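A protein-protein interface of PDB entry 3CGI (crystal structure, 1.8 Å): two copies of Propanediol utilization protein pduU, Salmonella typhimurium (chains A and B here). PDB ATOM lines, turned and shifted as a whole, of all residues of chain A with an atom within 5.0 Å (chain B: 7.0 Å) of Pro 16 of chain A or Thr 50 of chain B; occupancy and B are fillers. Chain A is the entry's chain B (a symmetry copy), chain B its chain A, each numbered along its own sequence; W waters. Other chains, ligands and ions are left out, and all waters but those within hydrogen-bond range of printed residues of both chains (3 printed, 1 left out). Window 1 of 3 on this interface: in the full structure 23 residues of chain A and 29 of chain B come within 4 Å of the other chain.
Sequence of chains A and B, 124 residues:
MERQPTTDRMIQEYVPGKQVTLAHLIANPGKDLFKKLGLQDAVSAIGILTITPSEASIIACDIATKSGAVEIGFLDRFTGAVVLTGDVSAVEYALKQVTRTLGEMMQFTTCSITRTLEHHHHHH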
ATOM      1  N   TYR A  14      -0.780  12.380  16.452  1.00  0.00           N
ATOM      2  CA  TYR A  14       0.232  13.128  15.760  1.00  0.00           C
ATOM      3  C   TYR A  14      -0.114  14.601  15.634  1.00  0.00           C
ATOM      4  O   TYR A  14      -1.271  14.954  15.442  1.00  0.00           O
ATOM      5  CB  TYR A  14       0.520  12.539  14.375  1.00  0.00           C
ATOM      6  CG  TYR A  14      -0.631  12.361  13.414  1.00  0.00           C
ATOM      7  CD1 TYR A  14      -1.297  11.133  13.306  1.00  0.00           C
ATOM      8  CD2 TYR A  14      -0.971  13.365  12.529  1.00  0.00           C
ATOM      9  CE1 TYR A  14      -2.324  10.948  12.386  1.00  0.00           C
ATOM     10  CE2 TYR A  14      -1.992  13.190  11.600  1.00  0.00           C
ATOM     11  CZ  TYR A  14      -2.655  11.981  11.529  1.00  0.00           C
ATOM     12  OH  TYR A  14      -3.665  11.830  10.605  1.00  0.00           O
ATOM     13  N   VAL A  15       0.905  15.436  15.825  1.00  0.00           N
ATOM     14  CA  VAL A  15       0.843  16.867  15.549  1.00  0.00           C
ATOM     15  C   VAL A  15       2.211  17.249  15.022  1.00  0.00           C
ATOM     16  O   VAL A  15       3.222  16.627  15.379  1.00  0.00           O
ATOM     17  CB  VAL A  15       0.493  17.725  16.799  1.00  0.00           C
ATOM     18  CG1 VAL A  15      -0.898  17.332  17.352  1.00  0.00           C
ATOM     19  CG2 VAL A  15       1.557  17.608  17.878  1.00  0.00           C
ATOM     20  N   PRO A  16       2.266  18.260  14.160  1.00  0.00           N
ATOM     21  CA  PRO A  16       3.576  18.703  13.728  1.00  0.00           C
ATOM     22  C   PRO A  16       4.351  19.401  14.841  1.00  0.00           C
ATOM     23  O   PRO A  16       3.775  20.109  15.684  1.00  0.00           O
ATOM     24  CB  PRO A  16       3.253  19.692  12.600  1.00  0.00           C
ATOM     25  CG  PRO A  16       1.964  20.224  12.958  1.00  0.00           C
ATOM     26  CD  PRO A  16       1.200  19.048  13.528  1.00  0.00           C
ATOM     27  N   GLY A  17       5.665  19.168  14.833  1.00  0.00           N
ATOM     28  CA  GLY A  17       6.598  19.904  15.646  1.00  0.00           C
ATOM     29  C   GLY A  17       6.884  21.260  15.034  1.00  0.00           C
ATOM     30  O   GLY A  17       6.396  21.600  13.941  1.00  0.00           O
ATOM     31  N   LYS A  18       7.698  22.030  15.731  1.00  0.00           N
ATOM     32  CA  LYS A  18       8.157  23.325  15.252  1.00  0.00           C
ATOM     33  C   LYS A  18       9.664  23.277  15.173  1.00  0.00           C
ATOM     34  O   LYS A  18      10.373  23.265  16.176  1.00  0.00           O
ATOM     35  CB  LYS A  18       7.699  24.443  16.154  1.00  0.00           C
ATOM     36  CG  LYS A  18       6.198  24.633  16.158  1.00  0.00           C
ATOM     37  CD  LYS A  18       5.748  25.549  17.284  1.00  0.00           C
ATOM     38  CE  LYS A  18       6.264  26.966  17.105  1.00  0.00           C
ATOM     39  NZ  LYS A  18       5.724  27.932  18.134  1.00  0.00           N
ATOM     40  N   THR A  52       9.229  22.483   9.634  1.00  0.00           N
ATOM     41  CA  THR A  52       8.013  21.898  10.133  1.00  0.00           C
ATOM     42  C   THR A  52       7.441  22.916  11.142  1.00  0.00           C
ATOM     43  O   THR A  52       8.178  23.460  11.956  1.00  0.00           O
ATOM     44  CB  THR A  52       8.276  20.565  10.852  1.00  0.00           C
ATOM     45  OG1 THR A  52       9.106  19.748  10.031  1.00  0.00           O
ATOM     46  CG2 THR A  52       6.978  19.861  11.150  1.00  0.00           C
ATOM     47  N   PRO A  53       6.129  23.173  11.089  1.00  0.00           N
ATOM     48  CA  PRO A  53       5.173  22.624  10.171  1.00  0.00           C
ATOM     49  C   PRO A  53       5.356  23.224   8.789  1.00  0.00           C
ATOM     50  O   PRO A  53       5.950  24.283   8.642  1.00  0.00           O
ATOM     51  CB  PRO A  53       3.821  23.081  10.748  1.00  0.00           C
ATOM     52  CG  PRO A  53       4.124  24.312  11.461  1.00  0.00           C
ATOM     53  CD  PRO A  53       5.501  24.122  12.036  1.00  0.00           C
ATOM     54  N   GLU A  55       3.602  24.856   6.753  1.00  0.00           N
ATOM     55  CA  GLU A  55       3.101  26.196   6.500  1.00  0.00           C
ATOM     56  C   GLU A  55       4.062  27.298   6.936  1.00  0.00           C
ATOM     57  O   GLU A  55       3.998  28.389   6.412  1.00  0.00           O
ATOM     58  CB  GLU A  55       1.736  26.416   7.158  1.00  0.00           C
ATOM     59  CG  GLU A  55       0.629  25.554   6.557  1.00  0.00           C
ATOM     60  CD  GLU A  55       0.650  24.111   7.020  1.00  0.00           C
ATOM     61  OE1 GLU A  55       1.309  23.782   8.046  1.00  0.00           O
ATOM     62  OE2 GLU A  55      -0.015  23.281   6.357  1.00  0.00           O
ATOM     63  N   GLN B  19      -4.878  20.197  17.474  1.00  0.00           N
ATOM     64  CA  GLN B  19      -3.918  21.279  17.732  1.00  0.00           C
ATOM     65  C   GLN B  19      -3.860  22.331  16.642  1.00  0.00           C
ATOM     66  O   GLN B  19      -3.860  22.016  15.457  1.00  0.00           O
ATOM     67  CB  GLN B  19      -2.527  20.681  17.920  1.00  0.00           C
ATOM     68  CG  GLN B  19      -1.412  21.681  18.181  1.00  0.00           C
ATOM     69  CD  GLN B  19      -0.122  21.022  18.596  1.00  0.00           C
ATOM     70  OE1 GLN B  19      -0.049  20.377  19.656  1.00  0.00           O
ATOM     71  NE2 GLN B  19       0.934  21.216  17.787  1.00  0.00           N
ATOM     72  N   VAL B  20      -3.815  23.597  17.069  1.00  0.00           N
ATOM     73  CA  VAL B  20      -3.488  24.707  16.176  1.00  0.00           C
ATOM     74  C   VAL B  20      -2.010  24.978  16.497  1.00  0.00           C
ATOM     75  O   VAL B  20      -1.667  25.407  17.613  1.00  0.00           O
ATOM     76  CB  VAL B  20      -4.370  25.928  16.433  1.00  0.00           C
ATOM     77  CG1 VAL B  20      -3.920  27.107  15.624  1.00  0.00           C
ATOM     78  CG2 VAL B  20      -5.854  25.607  16.127  1.00  0.00           C
ATOM     79  N   THR B  21      -1.136  24.630  15.560  1.00  0.00           N
ATOM     80  CA  THR B  21       0.326  24.720  15.783  1.00  0.00           C
ATOM     81  C   THR B  21       0.865  26.094  15.443  1.00  0.00           C
ATOM     82  O   THR B  21       1.790  26.572  16.089  1.00  0.00           O
ATOM     83  CB  THR B  21       1.080  23.666  14.942  1.00  0.00           C
ATOM     84  OG1 THR B  21       0.636  22.349  15.302  1.00  0.00           O
ATOM     85  CG2 THR B  21       2.618  23.783  15.090  1.00  0.00           C
ATOM     86  N   LEU B  22       0.315  26.696  14.378  1.00  0.00           N
ATOM     87  CA  LEU B  22       0.686  28.037  13.927  1.00  0.00           C
ATOM     88  C   LEU B  22      -0.559  28.935  13.758  1.00  0.00           C
ATOM     89  O   LEU B  22      -1.592  28.479  13.283  1.00  0.00           O
ATOM     90  CB  LEU B  22       1.393  27.910  12.578  1.00  0.00           C
ATOM     91  CG  LEU B  22       2.182  29.081  12.012  1.00  0.00           C
ATOM     92  CD1 LEU B  22       3.404  29.339  12.870  1.00  0.00           C
ATOM     93  CD2 LEU B  22       2.593  28.787  10.552  1.00  0.00           C
ATOM     94  N   ALA B  23      -0.448  30.190  14.172  1.00  0.00           N
ATOM     95  CA  ALA B  23      -1.490  31.227  13.994  1.00  0.00           C
ATOM     96  C   ALA B  23      -0.709  32.527  13.832  1.00  0.00           C
ATOM     97  O   ALA B  23      -0.466  33.212  14.790  1.00  0.00           O
ATOM     98  CB  ALA B  23      -2.417  31.291  15.193  1.00  0.00           C
ATOM     99  N   HIS B  24      -0.342  32.878  12.600  1.00  0.00           N
ATOM    100  CA  HIS B  24       0.682  33.875  12.391  1.00  0.00           C
ATOM    101  C   HIS B  24       0.250  34.941  11.445  1.00  0.00           C
ATOM    102  O   HIS B  24      -0.297  34.640  10.397  1.00  0.00           O
ATOM    103  CB  HIS B  24       1.939  33.206  11.825  1.00  0.00           C
ATOM    104  CG  HIS B  24       3.093  34.139  11.709  1.00  0.00           C
ATOM    105  ND1 HIS B  24       3.980  34.343  12.736  1.00  0.00           N
ATOM    106  CD2 HIS B  24       3.485  34.952  10.698  1.00  0.00           C
ATOM    107  CE1 HIS B  24       4.863  35.254  12.377  1.00  0.00           C
ATOM    108  NE2 HIS B  24       4.596  35.625  11.136  1.00  0.00           N
ATOM    109  N   ILE B  48      -2.028  32.964   8.851  1.00  0.00           N
ATOM    110  CA  ILE B  48      -1.599  31.624   8.447  1.00  0.00           C
ATOM    111  C   ILE B  48      -1.836  30.706   9.587  1.00  0.00           C
ATOM    112  O   ILE B  48      -1.339  30.981  10.661  1.00  0.00           O
ATOM    113  CB  ILE B  48      -0.081  31.614   8.066  1.00  0.00           C
ATOM    114  CG1 ILE B  48       0.197  32.584   6.902  1.00  0.00           C
ATOM    115  CG2 ILE B  48       0.361  30.216   7.654  1.00  0.00           C
ATOM    116  CD1 ILE B  48       1.523  33.325   7.044  1.00  0.00           C
ATOM    117  N   LEU B  49      -2.603  29.640   9.341  1.00  0.00           N
ATOM    118  CA  LEU B  49      -2.949  28.661  10.337  1.00  0.00           C
ATOM    119  C   LEU B  49      -2.441  27.266   9.954  1.00  0.00           C
ATOM    120  O   LEU B  49      -2.498  26.891   8.795  1.00  0.00           O
ATOM    121  CB  LEU B  49      -4.479  28.614  10.469  1.00  0.00           C
ATOM    122  CG  LEU B  49      -5.146  29.835  11.092  1.00  0.00           C
ATOM    123  CD1 LEU B  49      -6.623  29.991  10.718  1.00  0.00           C
ATOM    124  CD2 LEU B  49      -4.963  29.751  12.641  1.00  0.00           C
ATOM    125  N   THR B  50      -1.930  26.528  10.942  1.00  0.00           N
ATOM    126  CA  THR B  50      -1.595  25.117  10.819  1.00  0.00           C
ATOM    127  C   THR B  50      -2.491  24.416  11.809  1.00  0.00           C
ATOM    128  O   THR B  50      -2.392  24.678  13.026  1.00  0.00           O
ATOM    129  CB  THR B  50      -0.120  24.771  11.225  1.00  0.00           C
ATOM    130  OG1 THR B  50       0.797  25.367  10.297  1.00  0.00           O
ATOM    131  CG2 THR B  50       0.094  23.284  11.238  1.00  0.00           C
ATOM    132  N   ILE B  51      -3.311  23.495  11.297  1.00  0.00           N
ATOM    133  CA  ILE B  51      -4.334  22.841  12.082  1.00  0.00           C
ATOM    134  C   ILE B  51      -4.361  21.321  11.852  1.00  0.00           C
ATOM    135  O   ILE B  51      -4.319  20.867  10.704  1.00  0.00           O
ATOM    136  CB  ILE B  51      -5.713  23.405  11.679  1.00  0.00           C
ATOM    137  CG1 ILE B  51      -5.774  24.929  11.921  1.00  0.00           C
ATOM    138  CG2 ILE B  51      -6.834  22.676  12.411  1.00  0.00           C
ATOM    139  CD1 ILE B  51      -6.969  25.604  11.223  1.00  0.00           C
ATOM    140  N   THR B  52      -4.415  20.576  12.955  1.00  0.00           N
ATOM    141  CA  THR B  52      -4.640  19.145  12.951  1.00  0.00           C
ATOM    142  C   THR B  52      -5.856  18.867  13.846  1.00  0.00           C
ATOM    143  O   THR B  52      -5.976  19.458  14.920  1.00  0.00           O
ATOM    144  CB  THR B  52      -3.440  18.384  13.549  1.00  0.00           C
ATOM    145  OG1 THR B  52      -2.216  18.882  12.967  1.00  0.00           O
ATOM    146  CG2 THR B  52      -3.603  16.893  13.307  1.00  0.00           C
ATOM    147  N   THR B  79      -4.142  19.128   4.266  1.00  0.00           N
ATOM    148  CA  THR B  79      -3.038  19.394   5.180  1.00  0.00           C
ATOM    149  C   THR B  79      -3.439  20.176   6.444  1.00  0.00           C
ATOM    150  O   THR B  79      -2.676  20.197   7.409  1.00  0.00           O
ATOM    151  CB  THR B  79      -1.935  20.194   4.476  1.00  0.00           C
ATOM    152  OG1 THR B  79      -2.387  21.527   4.269  1.00  0.00           O
ATOM    153  CG2 THR B  79      -1.561  19.569   3.127  1.00  0.00           C
ATOM    154  N   GLY B  80      -4.609  20.823   6.431  1.00  0.00           N
ATOM    155  CA  GLY B  80      -5.078  21.632   7.561  1.00  0.00           C
ATOM    156  C   GLY B  80      -4.671  23.093   7.442  1.00  0.00           C
ATOM    157  O   GLY B  80      -4.961  23.899   8.334  1.00  0.00           O
ATOM    158  N   ALA B  81      -4.030  23.463   6.328  1.00  0.00           N
ATOM    159  CA  ALA B  81      -3.583  24.849   6.183  1.00  0.00           C
ATOM    160  C   ALA B  81      -4.733  25.763   5.796  1.00  0.00           C
ATOM    161  O   ALA B  81      -5.593  25.395   4.975  1.00  0.00           O
ATOM    162  CB  ALA B  81      -2.469  24.969   5.175  1.00  0.00           C
ATOM    163  N   VAL B  82      -4.731  26.955   6.393  1.00  0.00           N
ATOM    164  CA  VAL B  82      -5.654  28.027   6.034  1.00  0.00           C
ATOM    165  C   VAL B  82      -4.856  29.337   5.936  1.00  0.00           C
ATOM    166  O   VAL B  82      -4.066  29.624   6.787  1.00  0.00           O
ATOM    167  CB  VAL B  82      -6.794  28.183   7.070  1.00  0.00           C
ATOM    168  CG1 VAL B  82      -7.664  29.439   6.796  1.00  0.00           C
ATOM    169  CG2 VAL B  82      -7.673  26.904   7.160  1.00  0.00           C
ATOM    170  N   CYS B 111      -1.536  27.468  19.979  1.00  0.00           N
ATOM    171  CA  CYS B 111      -0.361  28.319  20.093  1.00  0.00           C
ATOM    172  C   CYS B 111      -0.813  29.764  20.325  1.00  0.00           C
ATOM    173  O   CYS B 111      -1.986  30.081  20.154  1.00  0.00           O
ATOM    174  CB  CYS B 111       0.393  28.269  18.807  1.00  0.00           C
ATOM    175  SG  CYS B 111      -0.664  28.709  17.396  1.00  0.00           S
HETATM  176  O   HOH W   1       3.881  20.765  18.228  1.00  0.00           O
HETATM  177  O   HOH W   2       0.034  23.406   3.744  1.00  0.00           O
HETATM  178  O   HOH W   3       3.448  28.806  16.685  1.00  0.00           O
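The backbone NH of Ala 81 of chain B sits at hydrogen-bond distance from the side-chain hydroxyl of Thr 79 of chain B, 3.3 Å away. NE2 of Gln 19 of chain B is in hydrogen-bond range of OG1 of Thr 21 of chain B, 2.7 Å away. The backbone NH (N) of Gln 19 of chain B lies within hydrogen-bond range of the backbone carbonyl oxygen (O) of Thr 52 of chain B, 2.9 Å away. N of Thr 21 of chain B sits at hydrogen-bond distance from O of Thr 50 of chain B (2.8 Å). The backbone NH (N) of Thr 50 of chain B sits at hydrogen-bond distance from the backbone carbonyl oxygen (O) of Leu 22 of chain B, at 3.1 Å. SG of Cys 111 of chain B lies close to O of Thr 21 of chain B, at 3.5 Å.
Along chain B the printed residues that touch a printed residue of chain A span positions 19 to 81. Of the 8 printed residues of chain A, 6 touch a printed residue of chain B. Hydrophobic or aromatic side chains of chain A within 4 Å of the printed part of chain B: Val 15, Pro 16 and Pro 53. Among the printed residues, 12 pairs touch across the chains. Among the printed residues, no Asp or Glu carboxylate lies within 4 Å of a Lys or Arg side-chain nitrogen of the other chain.
The side-chain carboxylate of Glu 55 of chain A is in hydrogen-bond range of the side-chain hydroxyl of Thr 50 of chain B (2.8 Å).
1 position is printed for both chains.
Water W2 bridges the side-chain carboxylate of Glu 55 of chain A (2.6 Å) and the side-chain hydroxyl of Thr 79 of chain B (3.1 Å). Water W1 bridges the backbone carbonyl oxygen (O) of Pro 16 of chain A (2.6 Å) and the side-chain amide nitrogen (NE2) of Gln 19 of chain B (3.0 Å). Water W3 lies within hydrogen-bond range of NZ of Lys 18 of chain A and O of Thr 21 of chain B.
Among the printed residues, merely in contact across the chains: Glu 55 of chain A with Ala 81 of chain B (3.2 Å), Pro 16 of chain A with Thr 21 of chain B (3.4 Å), Pro 16 of chain A with Thr 52 of chain B (3.5 Å), Glu 55 of chain A with Thr 79 of chain B (3.6 Å), Val 15 of chain A with Gln 19 of chain B (3.7 Å), Pro 53 of chain A with Thr 50 of chain B (3.7 Å), Pro 16 of chain A with Gln 19 of chain B (3.7 Å), Tyr 14 of chain A with Thr 52 of chain B (3.7 Å), Lys 18 of chain A with Thr 21 of chain B (3.8 Å), Pro 53 of chain A with Thr 21 of chain B (3.96 Å) and Pro 16 of chain A with Thr 50 of chain B (3.98 Å).
Of chain B, only Gln 19, Thr 21, Thr 50 and Thr 52 come within 4 Å of Pro 16 of chain A. Of chain A, only Pro 16, Pro 53 and Glu 55 come within 4 Å of Thr 50 of chain B. Of the printed residues of chain B, Pro 53 of chain A touches Thr 21 and Thr 50. Of the printed residues of chain B, Tyr 14 of chain A touches Thr 52. Val 82 of chain B touches none of the printed residues of chain A. The nearest residue of chain B that does not touch Pro 16 of chain A is Ile 51 of chain B (6.2 Å).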
